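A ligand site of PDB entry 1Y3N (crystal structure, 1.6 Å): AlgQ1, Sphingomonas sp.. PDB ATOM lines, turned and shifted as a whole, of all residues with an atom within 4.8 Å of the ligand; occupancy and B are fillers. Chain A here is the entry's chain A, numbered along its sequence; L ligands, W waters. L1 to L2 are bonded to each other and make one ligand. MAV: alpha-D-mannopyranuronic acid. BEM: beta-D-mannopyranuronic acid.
The backbone NH (N) of Ser 273 sits at hydrogen-bond distance from an oxygen (O6A) of BEM L2 (3.0 Å).
The guanidinium group (NH2) of Arg 20 is in salt-bridge range of an oxygen (O6A) of MAV L1, at 3.4 Å.
The side-chain hydroxyl (OG) of Ser 273 is in hydrogen-bond range of an oxygen (O6B) of BEM L2 (2.5 Å).
The guanidinium group of Arg 186 is in salt-bridge range of an oxygen (O6B) of BEM L2, 3.8 Å away.
The indole nitrogen of Trp 270 is in hydrogen-bond range of an oxygen (O2) of MAV L1.
An oxygen (O6A) of MAV L1 sits at hydrogen-bond distance from the side-chain hydroxyl of Tyr 129 (2.7 Å).
The side-chain hydroxyl (OH) of Tyr 395 lies within hydrogen-bond range of an oxygen (O3) of BEM L2.
O3 of BEM L2 sits at hydrogen-bond distance from OE1 of Glu 396, at 2.6 Å.
An oxygen (O6B) of BEM L2 lies within hydrogen-bond range of the side-chain amide nitrogen (ND2) of Asn 375 (3.0 Å).
The side-chain amide oxygen (OE1) of Gln 391 is in hydrogen-bond range of an oxygen (O3) of BEM L2, 3.1 Å away.
The guanidinium group (NH1) of Arg 137 lies close to the side-chain amide nitrogen (ND2) of Asn 206.
The backbone carbonyl oxygen (O) of Gln 384 is in hydrogen-bond range of the guanidinium group (NH1) of Arg 20 (3.4 Å).
The side-chain carboxylate (OD1) of Asp 187 lies within salt-bridge range of the guanidinium group (NH2) of Arg 137 (3.0 Å).
The guanidinium group (NH1) of Arg 309 lies within salt-bridge range of the side-chain carboxylate (OE1) of Glu 396.
The side-chain amide oxygen of Gln 391 sits close to the side-chain amide oxygen of Gln 384 (3.1 Å).
The backbone NH (N) of Arg 313 lies within hydrogen-bond range of the backbone carbonyl oxygen (O) of Tyr 129, at 3.0 Å.
The backbone carbonyl oxygen of Tyr 395 sits close to the indole nitrogen of Trp 399, at 3.1 Å.
The side-chain amide oxygen (OE1) of Gln 391 sits at hydrogen-bond distance from the side-chain hydroxyl (OH) of Tyr 129.
NH2 of Arg 137 touches O2 of MAV L1, 3.5 Å away.
CB of Ala 272 touches O6A of BEM L2 (3.4 Å).
NH1 of Arg 309 touches O3 of BEM L2, at 3.8 Å.
Tyr 379 touches the ligand.
CH2 of Trp 399 touches O6A of BEM L2 (3.7 Å).
Hydrophobic or aromatic side chains within 4 Å of the ligand: Tyr 129, Trp 270, Ala 272, Tyr 395 and Trp 399.
Within 4 Å of the ligand: Arg 20, Tyr 129, Arg 137, Arg 186, Trp 270, Ala 272, Ser 273, Arg 309, Asn 375, Tyr 379, Gln 391, Tyr 395, Glu 396 and Trp 399.
The nearest printed residue that does not touch the ligand is Asn 206 (4.4 Å).
Water W4 bridges an oxygen (O6B) of MAV L1 (2.6 Å) and the side-chain amide oxygen (OD1) of Asn 206 (2.9 Å).
Water W2 lies within hydrogen-bond range of O6A of BEM L2 (2.7 Å), OE2 of Glu 396 (2.9 Å) and N of Ala 272 (3.0 Å).
Water W7 lies within hydrogen-bond range of the side-chain carboxylate of Asp 187 (2.6 Å), an oxygen (O2) of MAV L1 (2.8 Å), the guanidinium group of Arg 186 (3.0 Å) and the guanidinium group of Arg 137 (3.4 Å).
Water W10 bridges O6B of MAV L1 (2.8 Å) and OH of Tyr 129 (3.3 Å).
Water W9 bridges an oxygen (O5) of MAV L1 (2.9 Å) and the guanidinium group (NH2) of Arg 313 (3.1 Å).
Water W8 lies within hydrogen-bond range of the guanidinium group of Arg 186 (3.0 Å), the side-chain hydroxyl of Tyr 379 (3.1 Å), the side-chain amide nitrogen of Asn 375 (3.4 Å) and an oxygen (O3) of MAV L1 (3.4 Å).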
ATOM      1  N   ARG A  20      -5.568  27.638  24.093  1.00  0.00           N
ATOM      2  CA  ARG A  20      -5.343  26.585  23.115  1.00  0.00           C
ATOM      3  C   ARG A  20      -4.086  26.768  22.288  1.00  0.00           C
ATOM      4  O   ARG A  20      -4.032  26.371  21.115  1.00  0.00           O
ATOM      5  CB  ARG A  20      -6.584  26.433  22.240  1.00  0.00           C
ATOM      6  CG  ARG A  20      -7.692  25.738  23.012  1.00  0.00           C
ATOM      7  CD  ARG A  20      -9.087  26.032  22.504  1.00  0.00           C
ATOM      8  NE  ARG A  20     -10.058  25.489  23.452  1.00  0.00           N
ATOM      9  CZ  ARG A  20     -11.350  25.807  23.478  1.00  0.00           C
ATOM     10  NH1 ARG A  20     -11.839  26.685  22.615  1.00  0.00           N
ATOM     11  NH2 ARG A  20     -12.137  25.266  24.402  1.00  0.00           N
ATOM     12  N   TYR A 129     -15.683  26.866  32.603  1.00  0.00           N
ATOM     13  CA  TYR A 129     -16.251  26.619  31.287  1.00  0.00           C
ATOM     14  C   TYR A 129     -17.043  25.353  31.624  1.00  0.00           C
ATOM     15  O   TYR A 129     -16.463  24.354  32.071  1.00  0.00           O
ATOM     16  CB  TYR A 129     -15.132  26.327  30.288  1.00  0.00           C
ATOM     17  CG  TYR A 129     -15.493  25.487  29.074  1.00  0.00           C
ATOM     18  CD1 TYR A 129     -16.778  25.521  28.518  1.00  0.00           C
ATOM     19  CD2 TYR A 129     -14.527  24.699  28.445  1.00  0.00           C
ATOM     20  CE1 TYR A 129     -17.088  24.776  27.359  1.00  0.00           C
ATOM     21  CE2 TYR A 129     -14.821  23.959  27.291  1.00  0.00           C
ATOM     22  CZ  TYR A 129     -16.109  24.004  26.754  1.00  0.00           C
ATOM     23  OH  TYR A 129     -16.393  23.277  25.615  1.00  0.00           O
ATOM     24  N   ARG A 137     -15.115  12.087  22.466  1.00  0.00           N
ATOM     25  CA  ARG A 137     -14.391  11.460  21.368  1.00  0.00           C
ATOM     26  C   ARG A 137     -14.813  10.030  21.053  1.00  0.00           C
ATOM     27  O   ARG A 137     -15.456   9.348  21.852  1.00  0.00           O
ATOM     28  CB  ARG A 137     -12.885  11.445  21.679  1.00  0.00           C
ATOM     29  CG  ARG A 137     -12.245  12.823  21.856  1.00  0.00           C
ATOM     30  CD  ARG A 137     -10.744  12.671  22.043  1.00  0.00           C
ATOM     31  NE  ARG A 137     -10.015  13.930  21.944  1.00  0.00           N
ATOM     32  CZ  ARG A 137      -9.893  14.817  22.926  1.00  0.00           C
ATOM     33  NH1 ARG A 137     -10.458  14.613  24.109  1.00  0.00           N
ATOM     34  NH2 ARG A 137      -9.155  15.912  22.740  1.00  0.00           N
ATOM     35  N   ARG A 186      -5.157  15.415  15.965  1.00  0.00           N
ATOM     36  CA  ARG A 186      -4.963  16.828  16.302  1.00  0.00           C
ATOM     37  C   ARG A 186      -4.234  16.987  17.636  1.00  0.00           C
ATOM     38  O   ARG A 186      -3.518  17.965  17.847  1.00  0.00           O
ATOM     39  CB  ARG A 186      -6.316  17.544  16.474  1.00  0.00           C
ATOM     40  CG  ARG A 186      -7.103  17.865  15.230  1.00  0.00           C
ATOM     41  CD  ARG A 186      -8.183  18.885  15.591  1.00  0.00           C
ATOM     42  NE  ARG A 186      -9.327  18.321  16.317  1.00  0.00           N
ATOM     43  CZ  ARG A 186     -10.231  19.050  16.965  1.00  0.00           C
ATOM     44  NH1 ARG A 186     -10.120  20.375  17.005  1.00  0.00           N
ATOM     45  NH2 ARG A 186     -11.278  18.469  17.546  1.00  0.00           N
ATOM     46  N   ASP A 187      -4.456  16.037  18.543  1.00  0.00           N
ATOM     47  CA  ASP A 187      -3.863  16.106  19.868  1.00  0.00           C
ATOM     48  C   ASP A 187      -2.734  15.128  20.076  1.00  0.00           C
ATOM     49  O   ASP A 187      -2.927  13.913  19.998  1.00  0.00           O
ATOM     50  CB  ASP A 187      -4.915  15.831  20.950  1.00  0.00           C
ATOM     51  CG  ASP A 187      -6.118  16.740  20.828  1.00  0.00           C
ATOM     52  OD1 ASP A 187      -7.196  16.246  20.442  1.00  0.00           O
ATOM     53  OD2 ASP A 187      -5.992  17.947  21.113  1.00  0.00           O
ATOM     54  N   ASN A 206     -11.347  13.925  30.865  1.00  0.00           N
ATOM     55  CA  ASN A 206     -11.106  14.756  29.682  1.00  0.00           C
ATOM     56  C   ASN A 206      -9.915  15.677  29.936  1.00  0.00           C
ATOM     57  O   ASN A 206      -9.371  16.265  28.998  1.00  0.00           O
ATOM     58  CB  ASN A 206     -12.350  15.584  29.357  1.00  0.00           C
ATOM     59  CG  ASN A 206     -12.221  16.355  28.041  1.00  0.00           C
ATOM     60  OD1 ASN A 206     -12.261  17.592  28.033  1.00  0.00           O
ATOM     61  ND2 ASN A 206     -12.066  15.634  26.938  1.00  0.00           N
ATOM     62  N   TRP A 270     -13.385  14.213  18.472  1.00  0.00           N
ATOM     63  CA  TRP A 270     -14.791  14.541  18.715  1.00  0.00           C
ATOM     64  C   TRP A 270     -15.690  14.190  17.541  1.00  0.00           C
ATOM     65  O   TRP A 270     -15.367  14.472  16.389  1.00  0.00           O
ATOM     66  CB  TRP A 270     -14.927  16.023  19.069  1.00  0.00           C
ATOM     67  CG  TRP A 270     -14.258  16.411  20.358  1.00  0.00           C
ATOM     68  CD1 TRP A 270     -12.922  16.503  20.603  1.00  0.00           C
ATOM     69  CD2 TRP A 270     -14.915  16.780  21.582  1.00  0.00           C
ATOM     70  NE1 TRP A 270     -12.692  16.916  21.901  1.00  0.00           N
ATOM     71  CE2 TRP A 270     -13.901  17.088  22.517  1.00  0.00           C
ATOM     72  CE3 TRP A 270     -16.255  16.885  21.976  1.00  0.00           C
ATOM     73  CZ2 TRP A 270     -14.188  17.488  23.836  1.00  0.00           C
ATOM     74  CZ3 TRP A 270     -16.540  17.291  23.282  1.00  0.00           C
ATOM     75  CH2 TRP A 270     -15.515  17.583  24.195  1.00  0.00           C
ATOM     76  N   PHE A 271     -16.832  13.574  17.847  1.00  0.00           N
ATOM     77  CA  PHE A 271     -17.775  13.130  16.821  1.00  0.00           C
ATOM     78  C   PHE A 271     -18.255  14.158  15.816  1.00  0.00           C
ATOM     79  O   PHE A 271     -18.182  13.926  14.602  1.00  0.00           O
ATOM     80  CB  PHE A 271     -18.984  12.484  17.503  1.00  0.00           C
ATOM     81  CG  PHE A 271     -18.710  11.125  18.090  1.00  0.00           C
ATOM     82  CD1 PHE A 271     -18.718   9.990  17.284  1.00  0.00           C
ATOM     83  CD2 PHE A 271     -18.447  10.979  19.447  1.00  0.00           C
ATOM     84  CE1 PHE A 271     -18.465   8.727  17.818  1.00  0.00           C
ATOM     85  CE2 PHE A 271     -18.195   9.711  19.994  1.00  0.00           C
ATOM     86  CZ  PHE A 271     -18.197   8.590  19.171  1.00  0.00           C
ATOM     87  N   ALA A 272     -18.749  15.297  16.288  1.00  0.00           N
ATOM     88  CA  ALA A 272     -19.294  16.326  15.400  1.00  0.00           C
ATOM     89  C   ALA A 272     -18.321  16.893  14.369  1.00  0.00           C
ATOM     90  O   ALA A 272     -18.563  16.795  13.171  1.00  0.00           O
ATOM     91  CB  ALA A 272     -19.910  17.466  16.224  1.00  0.00           C
ATOM     92  N   SER A 273     -17.223  17.482  14.831  1.00  0.00           N
ATOM     93  CA  SER A 273     -16.276  18.080  13.896  1.00  0.00           C
ATOM     94  C   SER A 273     -15.558  17.047  13.022  1.00  0.00           C
ATOM     95  O   SER A 273     -15.274  17.307  11.855  1.00  0.00           O
ATOM     96  CB  SER A 273     -15.241  18.933  14.639  1.00  0.00           C
ATOM     97  OG  SER A 273     -14.419  18.152  15.482  1.00  0.00           O
ATOM     98  N   ARG A 309     -17.172  13.855  28.040  1.00  0.00           N
ATOM     99  CA  ARG A 309     -17.298  15.278  28.299  1.00  0.00           C
ATOM    100  C   ARG A 309     -17.129  15.492  29.812  1.00  0.00           C
ATOM    101  O   ARG A 309     -17.686  14.738  30.605  1.00  0.00           O
ATOM    102  CB  ARG A 309     -18.659  15.784  27.818  1.00  0.00           C
ATOM    103  CG  ARG A 309     -18.614  17.188  27.240  1.00  0.00           C
ATOM    104  CD  ARG A 309     -19.833  17.513  26.376  1.00  0.00           C
ATOM    105  NE  ARG A 309     -19.875  16.775  25.111  1.00  0.00           N
ATOM    106  CZ  ARG A 309     -20.051  17.348  23.923  1.00  0.00           C
ATOM    107  NH1 ARG A 309     -20.177  18.662  23.822  1.00  0.00           N
ATOM    108  NH2 ARG A 309     -20.109  16.603  22.816  1.00  0.00           N
ATOM    109  N   ARG A 313     -15.022  21.880  33.120  1.00  0.00           N
ATOM    110  CA  ARG A 313     -13.662  21.738  32.611  1.00  0.00           C
ATOM    111  C   ARG A 313     -12.750  22.589  33.480  1.00  0.00           C
ATOM    112  O   ARG A 313     -13.206  23.525  34.138  1.00  0.00           O
ATOM    113  CB  ARG A 313     -13.570  22.256  31.172  1.00  0.00           C
ATOM    114  CG  ARG A 313     -13.984  21.293  30.085  1.00  0.00           C
ATOM    115  CD  ARG A 313     -12.807  20.428  29.694  1.00  0.00           C
ATOM    116  NE  ARG A 313     -11.603  21.213  29.462  1.00  0.00           N
ATOM    117  CZ  ARG A 313     -10.391  20.689  29.311  1.00  0.00           C
ATOM    118  NH1 ARG A 313     -10.236  19.377  29.370  1.00  0.00           N
ATOM    119  NH2 ARG A 313      -9.337  21.477  29.157  1.00  0.00           N
ATOM    120  N   ASN A 375     -17.520  24.869  15.480  1.00  0.00           N
ATOM    121  CA  ASN A 375     -16.857  25.368  16.686  1.00  0.00           C
ATOM    122  C   ASN A 375     -15.667  26.244  16.314  1.00  0.00           C
ATOM    123  O   ASN A 375     -15.398  27.243  16.981  1.00  0.00           O
ATOM    124  CB  ASN A 375     -16.493  24.229  17.660  1.00  0.00           C
ATOM    125  CG  ASN A 375     -15.663  23.103  17.037  1.00  0.00           C
ATOM    126  OD1 ASN A 375     -15.451  23.051  15.817  1.00  0.00           O
ATOM    127  ND2 ASN A 375     -15.208  22.189  17.889  1.00  0.00           N
ATOM    128  N   TYR A 379     -14.983  30.189  17.438  1.00  0.00           N
ATOM    129  CA  TYR A 379     -13.734  30.684  18.031  1.00  0.00           C
ATOM    130  C   TYR A 379     -13.334  31.986  17.339  1.00  0.00           C
ATOM    131  O   TYR A 379     -12.930  32.959  17.994  1.00  0.00           O
ATOM    132  CB  TYR A 379     -12.584  29.685  17.827  1.00  0.00           C
ATOM    133  CG  TYR A 379     -12.789  28.289  18.399  1.00  0.00           C
ATOM    134  CD1 TYR A 379     -12.051  27.216  17.898  1.00  0.00           C
ATOM    135  CD2 TYR A 379     -13.690  28.046  19.426  1.00  0.00           C
ATOM    136  CE1 TYR A 379     -12.198  25.934  18.409  1.00  0.00           C
ATOM    137  CE2 TYR A 379     -13.854  26.752  19.946  1.00  0.00           C
ATOM    138  CZ  TYR A 379     -13.107  25.701  19.424  1.00  0.00           C
ATOM    139  OH  TYR A 379     -13.258  24.419  19.905  1.00  0.00           O
ATOM    140  N   GLN A 384     -17.755  30.062  22.061  1.00  0.00           N
ATOM    141  CA  GLN A 384     -17.202  28.747  22.388  1.00  0.00           C
ATOM    142  C   GLN A 384     -15.761  28.856  22.879  1.00  0.00           C
ATOM    143  O   GLN A 384     -14.946  27.948  22.654  1.00  0.00           O
ATOM    144  CB  GLN A 384     -17.280  27.810  21.179  1.00  0.00           C
ATOM    145  CG  GLN A 384     -18.704  27.463  20.718  1.00  0.00           C
ATOM    146  CD  GLN A 384     -19.554  26.833  21.804  1.00  0.00           C
ATOM    147  OE1 GLN A 384     -19.057  26.073  22.643  1.00  0.00           O
ATOM    148  NE2 GLN A 384     -20.848  27.135  21.793  1.00  0.00           N
ATOM    149  N   GLN A 391     -22.013  26.091  28.235  1.00  0.00           N
ATOM    150  CA  GLN A 391     -22.231  25.591  26.893  1.00  0.00           C
ATOM    151  C   GLN A 391     -23.657  25.054  26.767  1.00  0.00           C
ATOM    152  O   GLN A 391     -24.224  24.561  27.728  1.00  0.00           O
ATOM    153  CB  GLN A 391     -21.223  24.474  26.581  1.00  0.00           C
ATOM    154  CG  GLN A 391     -21.132  24.161  25.092  1.00  0.00           C
ATOM    155  CD  GLN A 391     -20.066  23.123  24.784  1.00  0.00           C
ATOM    156  OE1 GLN A 391     -19.327  23.254  23.806  1.00  0.00           O
ATOM    157  NE2 GLN A 391     -20.001  22.091  25.593  1.00  0.00           N
ATOM    158  N   TYR A 395     -26.419  24.109  20.354  1.00  0.00           N
ATOM    159  CA  TYR A 395     -25.536  24.730  19.368  1.00  0.00           C
ATOM    160  C   TYR A 395     -24.821  23.656  18.560  1.00  0.00           C
ATOM    161  O   TYR A 395     -24.642  23.783  17.354  1.00  0.00           O
ATOM    162  CB  TYR A 395     -24.501  25.635  20.064  1.00  0.00           C
ATOM    163  CG  TYR A 395     -23.053  25.134  19.997  1.00  0.00           C
ATOM    164  CD1 TYR A 395     -22.222  25.485  18.940  1.00  0.00           C
ATOM    165  CD2 TYR A 395     -22.539  24.305  21.002  1.00  0.00           C
ATOM    166  CE1 TYR A 395     -20.900  25.027  18.878  1.00  0.00           C
ATOM    167  CE2 TYR A 395     -21.218  23.841  20.953  1.00  0.00           C
ATOM    168  CZ  TYR A 395     -20.407  24.199  19.889  1.00  0.00           C
ATOM    169  OH  TYR A 395     -19.090  23.749  19.838  1.00  0.00           O
ATOM    170  N   GLU A 396     -24.434  22.585  19.249  1.00  0.00           N
ATOM    171  CA  GLU A 396     -23.712  21.477  18.622  1.00  0.00           C
ATOM    172  C   GLU A 396     -24.613  20.550  17.815  1.00  0.00           C
ATOM    173  O   GLU A 396     -24.216  20.052  16.760  1.00  0.00           O
ATOM    174  CB  GLU A 396     -22.995  20.675  19.708  1.00  0.00           C
ATOM    175  CG  GLU A 396     -21.942  19.709  19.189  1.00  0.00           C
ATOM    176  CD  GLU A 396     -21.196  19.028  20.308  1.00  0.00           C
ATOM    177  OE1 GLU A 396     -20.918  19.692  21.326  1.00  0.00           O
ATOM    178  OE2 GLU A 396     -20.851  17.832  20.168  1.00  0.00           O
ATOM    179  N   TRP A 399     -25.065  21.063  14.010  1.00  0.00           N
ATOM    180  CA  TRP A 399     -24.046  20.691  13.043  1.00  0.00           C
ATOM    181  C   TRP A 399     -23.473  19.277  13.251  1.00  0.00           C
ATOM    182  O   TRP A 399     -22.372  18.962  12.784  1.00  0.00           O
ATOM    183  CB  TRP A 399     -22.908  21.724  12.968  1.00  0.00           C
ATOM    184  CG  TRP A 399     -22.256  22.079  14.271  1.00  0.00           C
ATOM    185  CD1 TRP A 399     -22.738  22.916  15.225  1.00  0.00           C
ATOM    186  CD2 TRP A 399     -20.965  21.637  14.734  1.00  0.00           C
ATOM    187  NE1 TRP A 399     -21.842  23.037  16.258  1.00  0.00           N
ATOM    188  CE2 TRP A 399     -20.749  22.257  15.989  1.00  0.00           C
ATOM    189  CE3 TRP A 399     -19.991  20.775  14.221  1.00  0.00           C
ATOM    190  CZ2 TRP A 399     -19.576  22.045  16.727  1.00  0.00           C
ATOM    191  CZ3 TRP A 399     -18.818  20.563  14.959  1.00  0.00           C
ATOM    192  CH2 TRP A 399     -18.635  21.208  16.206  1.00  0.00           C
HETATM  193  C1  MAV L   1     -10.066  21.071  22.544  1.00  0.00           C
HETATM  194  O1  MAV L   1      -9.824  22.393  22.208  1.00  0.00           O
HETATM  195  C2  MAV L   1     -10.555  20.298  21.307  1.00  0.00           C
HETATM  196  O2  MAV L   1     -10.611  18.906  21.594  1.00  0.00           O
HETATM  197  C3  MAV L   1     -11.931  20.790  20.856  1.00  0.00           C
HETATM  198  O3  MAV L   1     -12.427  19.932  19.830  1.00  0.00           O
HETATM  199  C4  MAV L   1     -12.899  20.795  22.040  1.00  0.00           C
HETATM  200  O4  MAV L   1     -14.155  21.393  21.674  1.00  0.00           O
HETATM  201  C5  MAV L   1     -12.313  21.619  23.179  1.00  0.00           C
HETATM  202  O5  MAV L   1     -11.061  21.043  23.593  1.00  0.00           O
HETATM  203  C6  MAV L   1     -13.274  21.699  24.350  1.00  0.00           C
HETATM  204  O6A MAV L   1     -14.209  22.537  24.274  1.00  0.00           O
HETATM  205  O6B MAV L   1     -13.128  20.926  25.322  1.00  0.00           O
HETATM  206  C1  BEM L   2     -15.248  20.566  21.472  1.00  0.00           C
HETATM  207  C2  BEM L   2     -16.505  21.428  21.651  1.00  0.00           C
HETATM  208  O2  BEM L   2     -16.403  22.584  20.853  1.00  0.00           O
HETATM  209  C3  BEM L   2     -17.699  20.629  21.201  1.00  0.00           C
HETATM  210  O3  BEM L   2     -18.926  21.321  21.385  1.00  0.00           O
HETATM  211  C4  BEM L   2     -17.546  19.863  19.939  1.00  0.00           C
HETATM  212  C5  BEM L   2     -16.244  19.363  19.591  1.00  0.00           C
HETATM  213  O5  BEM L   2     -15.118  20.085  20.116  1.00  0.00           O
HETATM  214  C6  BEM L   2     -16.058  18.895  18.247  1.00  0.00           C
HETATM  215  O6B BEM L   2     -14.983  19.201  17.679  1.00  0.00           O
HETATM  216  O6A BEM L   2     -16.968  18.251  17.688  1.00  0.00           O
HETATM  217  O   HOH W   1      -7.722  19.440  19.442  1.00  0.00           O
HETATM  218  O   HOH W   2     -18.585  16.560  18.949  1.00  0.00           O
HETATM  219  O   HOH W   3     -14.749  24.225  22.139  1.00  0.00           O
HETATM  220  O   HOH W   4     -11.295  19.074  25.774  1.00  0.00           O
HETATM  221  O   HOH W   5      -9.490  23.549  19.477  1.00  0.00           O
HETATM  222  O   HOH W   6      -8.037  22.876  25.119  1.00  0.00           O
HETATM  223  O   HOH W   7      -9.455  17.332  19.642  1.00  0.00           O
HETATM  224  O   HOH W   8     -11.870  22.628  17.845  1.00  0.00           O
HETATM  225  O   HOH W   9      -9.604  21.180  26.096  1.00  0.00           O
HETATM  226  O   HOH W  10     -15.524  20.274  26.684  1.00  0.00           O
